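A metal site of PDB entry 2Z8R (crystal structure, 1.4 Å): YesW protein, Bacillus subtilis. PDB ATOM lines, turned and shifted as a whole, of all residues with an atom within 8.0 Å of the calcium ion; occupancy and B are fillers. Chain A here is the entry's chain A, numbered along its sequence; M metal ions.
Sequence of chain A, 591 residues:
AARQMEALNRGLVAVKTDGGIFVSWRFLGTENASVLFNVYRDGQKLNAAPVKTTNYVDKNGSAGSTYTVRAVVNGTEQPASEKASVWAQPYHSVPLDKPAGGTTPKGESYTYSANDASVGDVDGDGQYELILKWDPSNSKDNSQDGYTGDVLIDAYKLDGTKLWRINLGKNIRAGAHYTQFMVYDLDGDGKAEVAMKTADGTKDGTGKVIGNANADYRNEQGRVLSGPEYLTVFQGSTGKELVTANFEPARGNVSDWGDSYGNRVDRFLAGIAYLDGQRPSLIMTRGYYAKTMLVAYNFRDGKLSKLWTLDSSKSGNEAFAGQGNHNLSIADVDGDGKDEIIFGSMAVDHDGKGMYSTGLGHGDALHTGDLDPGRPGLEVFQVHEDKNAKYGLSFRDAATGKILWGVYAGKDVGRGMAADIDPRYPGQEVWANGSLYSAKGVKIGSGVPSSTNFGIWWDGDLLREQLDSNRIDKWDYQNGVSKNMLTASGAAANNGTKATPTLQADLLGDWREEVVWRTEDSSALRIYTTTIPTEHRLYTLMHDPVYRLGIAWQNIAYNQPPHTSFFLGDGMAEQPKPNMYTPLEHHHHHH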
ATOM      1  N   GLN A   4      -5.871  15.121 -12.182  1.00  0.00           N
ATOM      2  CA  GLN A   4      -5.430  16.392 -11.633  1.00  0.00           C
ATOM      3  C   GLN A   4      -4.256  16.907 -12.448  1.00  0.00           C
ATOM      4  O   GLN A   4      -3.262  16.192 -12.615  1.00  0.00           O
ATOM      5  CB  GLN A   4      -4.994  16.203 -10.186  1.00  0.00           C
ATOM      6  CG  GLN A   4      -4.519  17.485  -9.510  1.00  0.00           C
ATOM      7  CD  GLN A   4      -3.660  17.200  -8.302  1.00  0.00           C
ATOM      8  OE1 GLN A   4      -4.127  16.578  -7.341  1.00  0.00           O
ATOM      9  NE2 GLN A   4      -2.399  17.620  -8.355  1.00  0.00           N
ATOM     10  N   ASP A 121       4.653  25.078  -9.618  1.00  0.00           N
ATOM     11  CA  ASP A 121       4.044  26.358  -9.313  1.00  0.00           C
ATOM     12  C   ASP A 121       3.777  26.361  -7.808  1.00  0.00           C
ATOM     13  O   ASP A 121       2.787  25.792  -7.341  1.00  0.00           O
ATOM     14  CB  ASP A 121       2.742  26.521 -10.109  1.00  0.00           C
ATOM     15  CG  ASP A 121       2.036  27.833  -9.832  1.00  0.00           C
ATOM     16  OD1 ASP A 121       2.664  28.734  -9.246  1.00  0.00           O
ATOM     17  OD2 ASP A 121       0.859  27.949 -10.205  1.00  0.00           O
ATOM     18  N   VAL A 122       4.696  26.965  -7.055  1.00  0.00           N
ATOM     19  CA  VAL A 122       4.646  26.860  -5.596  1.00  0.00           C
ATOM     20  C   VAL A 122       3.640  27.815  -4.950  1.00  0.00           C
ATOM     21  O   VAL A 122       3.244  27.607  -3.796  1.00  0.00           O
ATOM     22  CB  VAL A 122       6.048  27.050  -4.950  1.00  0.00           C
ATOM     23  CG1 VAL A 122       7.059  26.086  -5.564  1.00  0.00           C
ATOM     24  CG2 VAL A 122       6.521  28.511  -5.042  1.00  0.00           C
ATOM     25  N   TYR A 184       6.027  18.710  -7.178  1.00  0.00           N
ATOM     26  CA  TYR A 184       4.689  18.408  -7.650  1.00  0.00           C
ATOM     27  C   TYR A 184       3.656  18.820  -6.643  1.00  0.00           C
ATOM     28  O   TYR A 184       3.931  18.828  -5.444  1.00  0.00           O
ATOM     29  CB  TYR A 184       4.542  16.893  -7.931  1.00  0.00           C
ATOM     30  CG  TYR A 184       3.632  16.620  -9.105  1.00  0.00           C
ATOM     31  CD1 TYR A 184       4.132  16.676 -10.404  1.00  0.00           C
ATOM     32  CD2 TYR A 184       2.285  16.323  -8.937  1.00  0.00           C
ATOM     33  CE1 TYR A 184       3.321  16.438 -11.511  1.00  0.00           C
ATOM     34  CE2 TYR A 184       1.443  16.093 -10.050  1.00  0.00           C
ATOM     35  CZ  TYR A 184       1.979  16.153 -11.325  1.00  0.00           C
ATOM     36  OH  TYR A 184       1.185  15.926 -12.423  1.00  0.00           O
ATOM     37  N   ASP A 185       2.459  19.151  -7.123  1.00  0.00           N
ATOM     38  CA  ASP A 185       1.338  19.363  -6.237  1.00  0.00           C
ATOM     39  C   ASP A 185       0.758  18.003  -5.842  1.00  0.00           C
ATOM     40  O   ASP A 185      -0.178  17.502  -6.467  1.00  0.00           O
ATOM     41  CB  ASP A 185       0.290  20.242  -6.917  1.00  0.00           C
ATOM     42  CG  ASP A 185      -0.909  20.519  -6.027  1.00  0.00           C
ATOM     43  OD1 ASP A 185      -0.826  20.282  -4.797  1.00  0.00           O
ATOM     44  OD2 ASP A 185      -1.954  20.964  -6.561  1.00  0.00           O
ATOM     45  N   LEU A 186       1.344  17.419  -4.807  1.00  0.00           N
ATOM     46  CA  LEU A 186       0.983  16.080  -4.371  1.00  0.00           C
ATOM     47  C   LEU A 186      -0.396  15.989  -3.733  1.00  0.00           C
ATOM     48  O   LEU A 186      -1.091  14.993  -3.896  1.00  0.00           O
ATOM     49  CB  LEU A 186       2.026  15.534  -3.397  1.00  0.00           C
ATOM     50  CG  LEU A 186       3.343  15.049  -4.023  1.00  0.00           C
ATOM     51  CD1 LEU A 186       4.390  14.877  -2.925  1.00  0.00           C
ATOM     52  CD2 LEU A 186       3.133  13.737  -4.767  1.00  0.00           C
ATOM     53  N   ASP A 187      -0.783  17.036  -2.998  1.00  0.00           N
ATOM     54  CA  ASP A 187      -2.061  16.988  -2.267  1.00  0.00           C
ATOM     55  C   ASP A 187      -3.246  17.631  -2.985  1.00  0.00           C
ATOM     56  O   ASP A 187      -4.393  17.503  -2.529  1.00  0.00           O
ATOM     57  CB  ASP A 187      -1.912  17.514  -0.823  1.00  0.00           C
ATOM     58  CG  ASP A 187      -1.499  18.967  -0.757  1.00  0.00           C
ATOM     59  OD1 ASP A 187      -1.407  19.614  -1.821  1.00  0.00           O
ATOM     60  OD2 ASP A 187      -1.261  19.455   0.360  1.00  0.00           O
ATOM     61  N   GLY A 188      -2.990  18.316  -4.096  1.00  0.00           N
ATOM     62  CA  GLY A 188      -4.051  18.841  -4.949  1.00  0.00           C
ATOM     63  C   GLY A 188      -4.686  20.131  -4.503  1.00  0.00           C
ATOM     64  O   GLY A 188      -5.875  20.357  -4.766  1.00  0.00           O
ATOM     65  N   ASP A 189      -3.910  20.996  -3.842  1.00  0.00           N
ATOM     66  CA  ASP A 189      -4.423  22.312  -3.426  1.00  0.00           C
ATOM     67  C   ASP A 189      -4.065  23.439  -4.401  1.00  0.00           C
ATOM     68  O   ASP A 189      -4.427  24.600  -4.173  1.00  0.00           O
ATOM     69  CB  ASP A 189      -3.958  22.662  -2.005  1.00  0.00           C
ATOM     70  CG  ASP A 189      -2.486  23.034  -1.936  1.00  0.00           C
ATOM     71  OD1 ASP A 189      -1.707  22.599  -2.816  1.00  0.00           O
ATOM     72  OD2 ASP A 189      -2.108  23.763  -0.991  1.00  0.00           O
ATOM     73  N   GLY A 190      -3.349  23.095  -5.464  1.00  0.00           N
ATOM     74  CA  GLY A 190      -2.942  24.064  -6.478  1.00  0.00           C
ATOM     75  C   GLY A 190      -1.511  24.590  -6.346  1.00  0.00           C
ATOM     76  O   GLY A 190      -1.051  25.370  -7.176  1.00  0.00           O
ATOM     77  N   LYS A 191      -0.804  24.131  -5.313  1.00  0.00           N
ATOM     78  CA  LYS A 191       0.554  24.589  -5.017  1.00  0.00           C
ATOM     79  C   LYS A 191       1.528  23.412  -4.922  1.00  0.00           C
ATOM     80  O   LYS A 191       1.230  22.418  -4.256  1.00  0.00           O
ATOM     81  CB  LYS A 191       0.570  25.388  -3.714  1.00  0.00           C
ATOM     82  CG  LYS A 191      -0.426  26.556  -3.707  1.00  0.00           C
ATOM     83  CD  LYS A 191      -0.313  27.380  -2.431  1.00  0.00           C
ATOM     84  CE  LYS A 191      -1.107  28.681  -2.556  1.00  0.00           C
ATOM     85  NZ  LYS A 191      -0.792  29.616  -1.442  1.00  0.00           N
ATOM     86  N   ALA A 192       2.671  23.513  -5.593  1.00  0.00           N
ATOM     87  CA  ALA A 192       3.655  22.424  -5.593  1.00  0.00           C
ATOM     88  C   ALA A 192       4.377  22.333  -4.256  1.00  0.00           C
ATOM     89  O   ALA A 192       4.628  23.352  -3.599  1.00  0.00           O
ATOM     90  CB  ALA A 192       4.661  22.625  -6.702  1.00  0.00           C
ATOM     91  N   GLU A 193       4.685  21.099  -3.868  1.00  0.00           N
ATOM     92  CA  GLU A 193       5.658  20.857  -2.799  1.00  0.00           C
ATOM     93  C   GLU A 193       6.897  20.168  -3.353  1.00  0.00           C
ATOM     94  O   GLU A 193       6.946  19.824  -4.550  1.00  0.00           O
ATOM     95  CB  GLU A 193       5.066  20.084  -1.612  1.00  0.00           C
ATOM     96  CG  GLU A 193       3.925  19.145  -1.930  1.00  0.00           C
ATOM     97  CD  GLU A 193       2.572  19.846  -2.146  1.00  0.00           C
ATOM     98  OE1 GLU A 193       1.674  19.198  -2.709  1.00  0.00           O
ATOM     99  OE2 GLU A 193       2.394  21.038  -1.772  1.00  0.00           O
ATOM    100  N   VAL A 194       7.915  20.022  -2.512  1.00  0.00           N
ATOM    101  CA  VAL A 194       9.183  19.413  -2.924  1.00  0.00           C
ATOM    102  C   VAL A 194       9.474  18.261  -1.978  1.00  0.00           C
ATOM    103  O   VAL A 194       9.462  18.433  -0.764  1.00  0.00           O
ATOM    104  CB  VAL A 194      10.356  20.440  -2.875  1.00  0.00           C
ATOM    105  CG1 VAL A 194      11.655  19.798  -3.370  1.00  0.00           C
ATOM    106  CG2 VAL A 194      10.004  21.678  -3.691  1.00  0.00           C
ATOM    107  N   VAL A 233       8.644  15.915   2.922  1.00  0.00           N
ATOM    108  CA  VAL A 233       7.897  16.790   2.027  1.00  0.00           C
ATOM    109  C   VAL A 233       8.043  18.210   2.561  1.00  0.00           C
ATOM    110  O   VAL A 233       7.726  18.473   3.733  1.00  0.00           O
ATOM    111  CB  VAL A 233       6.404  16.399   1.944  1.00  0.00           C
ATOM    112  CG1 VAL A 233       5.670  17.309   0.956  1.00  0.00           C
ATOM    113  CG2 VAL A 233       6.253  14.961   1.514  1.00  0.00           C
ATOM    114  N   PHE A 234       8.509  19.117   1.707  1.00  0.00           N
ATOM    115  CA  PHE A 234       8.735  20.517   2.043  1.00  0.00           C
ATOM    116  C   PHE A 234       7.692  21.382   1.336  1.00  0.00           C
ATOM    117  O   PHE A 234       7.335  21.101   0.179  1.00  0.00           O
ATOM    118  CB  PHE A 234      10.107  20.984   1.560  1.00  0.00           C
ATOM    119  CG  PHE A 234      11.290  20.312   2.220  1.00  0.00           C
ATOM    120  CD1 PHE A 234      11.826  20.799   3.404  1.00  0.00           C
ATOM    121  CD2 PHE A 234      11.892  19.189   1.630  1.00  0.00           C
ATOM    122  CE1 PHE A 234      12.926  20.197   4.002  1.00  0.00           C
ATOM    123  CE2 PHE A 234      12.998  18.577   2.214  1.00  0.00           C
ATOM    124  CZ  PHE A 234      13.520  19.079   3.389  1.00  0.00           C
ATOM    125  N   GLN A 235       7.252  22.451   1.997  1.00  0.00           N
ATOM    126  CA  GLN A 235       6.351  23.429   1.402  1.00  0.00           C
ATOM    127  C   GLN A 235       7.045  24.142   0.244  1.00  0.00           C
ATOM    128  O   GLN A 235       8.164  24.634   0.381  1.00  0.00           O
ATOM    129  CB  GLN A 235       5.914  24.424   2.472  1.00  0.00           C
ATOM    130  CG  GLN A 235       4.848  25.431   2.008  1.00  0.00           C
ATOM    131  CD  GLN A 235       4.351  26.289   3.149  1.00  0.00           C
ATOM    132  OE1 GLN A 235       5.111  26.694   4.018  1.00  0.00           O
ATOM    133  NE2 GLN A 235       3.053  26.592   3.143  1.00  0.00           N
ATOM    134  N   GLY A 236       6.377  24.184  -0.906  1.00  0.00           N
ATOM    135  CA  GLY A 236       6.993  24.721  -2.105  1.00  0.00           C
ATOM    136  C   GLY A 236       7.326  26.200  -2.008  1.00  0.00           C
ATOM    137  O   GLY A 236       8.331  26.651  -2.552  1.00  0.00           O
ATOM    138  N   LEU A 242       7.174  20.074   6.009  1.00  0.00           N
ATOM    139  CA  LEU A 242       5.775  19.780   6.309  1.00  0.00           C
ATOM    140  C   LEU A 242       5.664  18.483   7.096  1.00  0.00           C
ATOM    141  O   LEU A 242       5.033  18.440   8.170  1.00  0.00           O
ATOM    142  CB  LEU A 242       4.943  19.687   5.020  1.00  0.00           C
ATOM    143  CG  LEU A 242       4.693  21.030   4.323  1.00  0.00           C
ATOM    144  CD1 LEU A 242       4.086  20.819   2.951  1.00  0.00           C
ATOM    145  CD2 LEU A 242       3.804  21.930   5.194  1.00  0.00           C
ATOM    146  N   PHE A 299       0.891  11.999  -0.420  1.00  0.00           N
ATOM    147  CA  PHE A 299       0.871  13.134   0.496  1.00  0.00           C
ATOM    148  C   PHE A 299      -0.435  13.871   0.241  1.00  0.00           C
ATOM    149  O   PHE A 299      -0.586  14.545  -0.771  1.00  0.00           O
ATOM    150  CB  PHE A 299       2.084  14.051   0.320  1.00  0.00           C
ATOM    151  CG  PHE A 299       2.049  15.257   1.216  1.00  0.00           C
ATOM    152  CD1 PHE A 299       2.246  15.127   2.593  1.00  0.00           C
ATOM    153  CD2 PHE A 299       1.774  16.514   0.690  1.00  0.00           C
ATOM    154  CE1 PHE A 299       2.194  16.261   3.431  1.00  0.00           C
ATOM    155  CE2 PHE A 299       1.708  17.641   1.510  1.00  0.00           C
ATOM    156  CZ  PHE A 299       1.929  17.513   2.883  1.00  0.00           C
ATOM    157  N   PRO A 583      -7.014  21.875  -9.603  1.00  0.00           N
ATOM    158  CA  PRO A 583      -7.510  22.128  -8.242  1.00  0.00           C
ATOM    159  C   PRO A 583      -8.329  23.409  -8.134  1.00  0.00           C
ATOM    160  O   PRO A 583      -9.175  23.516  -7.243  1.00  0.00           O
ATOM    161  CB  PRO A 583      -6.231  22.243  -7.416  1.00  0.00           C
ATOM    162  CG  PRO A 583      -5.213  21.453  -8.202  1.00  0.00           C
ATOM    163  CD  PRO A 583      -5.541  21.749  -9.628  1.00  0.00           C
HETATM  164 CA    CA M   1       0.130  21.151  -2.709  1.00  0.00          CA
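Along chain A the residues within 4 Å of the calcium ion span positions 185 to 193.
The nearest printed residue that does not touch the calcium ion is Gly 188 (4.4 Å).
The backbone NH of Glu 193 sits at hydrogen-bond distance from the backbone carbonyl oxygen of Tyr 184.
The backbone carbonyl oxygen (O) of Asp 185 sits at hydrogen-bond distance from the side-chain amide nitrogen (NE2) of Gln 4, 2.9 Å away.
The backbone NH (N) of Leu 186 sits close to the side-chain carboxylate (OE1) of Glu 193 (2.8 Å).
The backbone NH (N) of Gly 188 sits close to the side-chain carboxylate (OD1) of Asp 185 (3.0 Å).
OD2 of Asp 185 sits at hydrogen-bond distance from N of Gly 190, at 2.8 Å.
O of Phe 299 sits close to N of Asp 187 (3.3 Å).
The calcium ion is bound by O of Lys 191 (2.3 Å), OD1 of Asp 189 (2.3 Å), OD1 of Asp 187 (2.3 Å), OE2 of Glu 193 (2.5 Å), OD1 of Asp 185 (2.5 Å) and OE1 of Glu 193 (2.5 Å).
The calcium ion has six donor atoms within binding distance.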
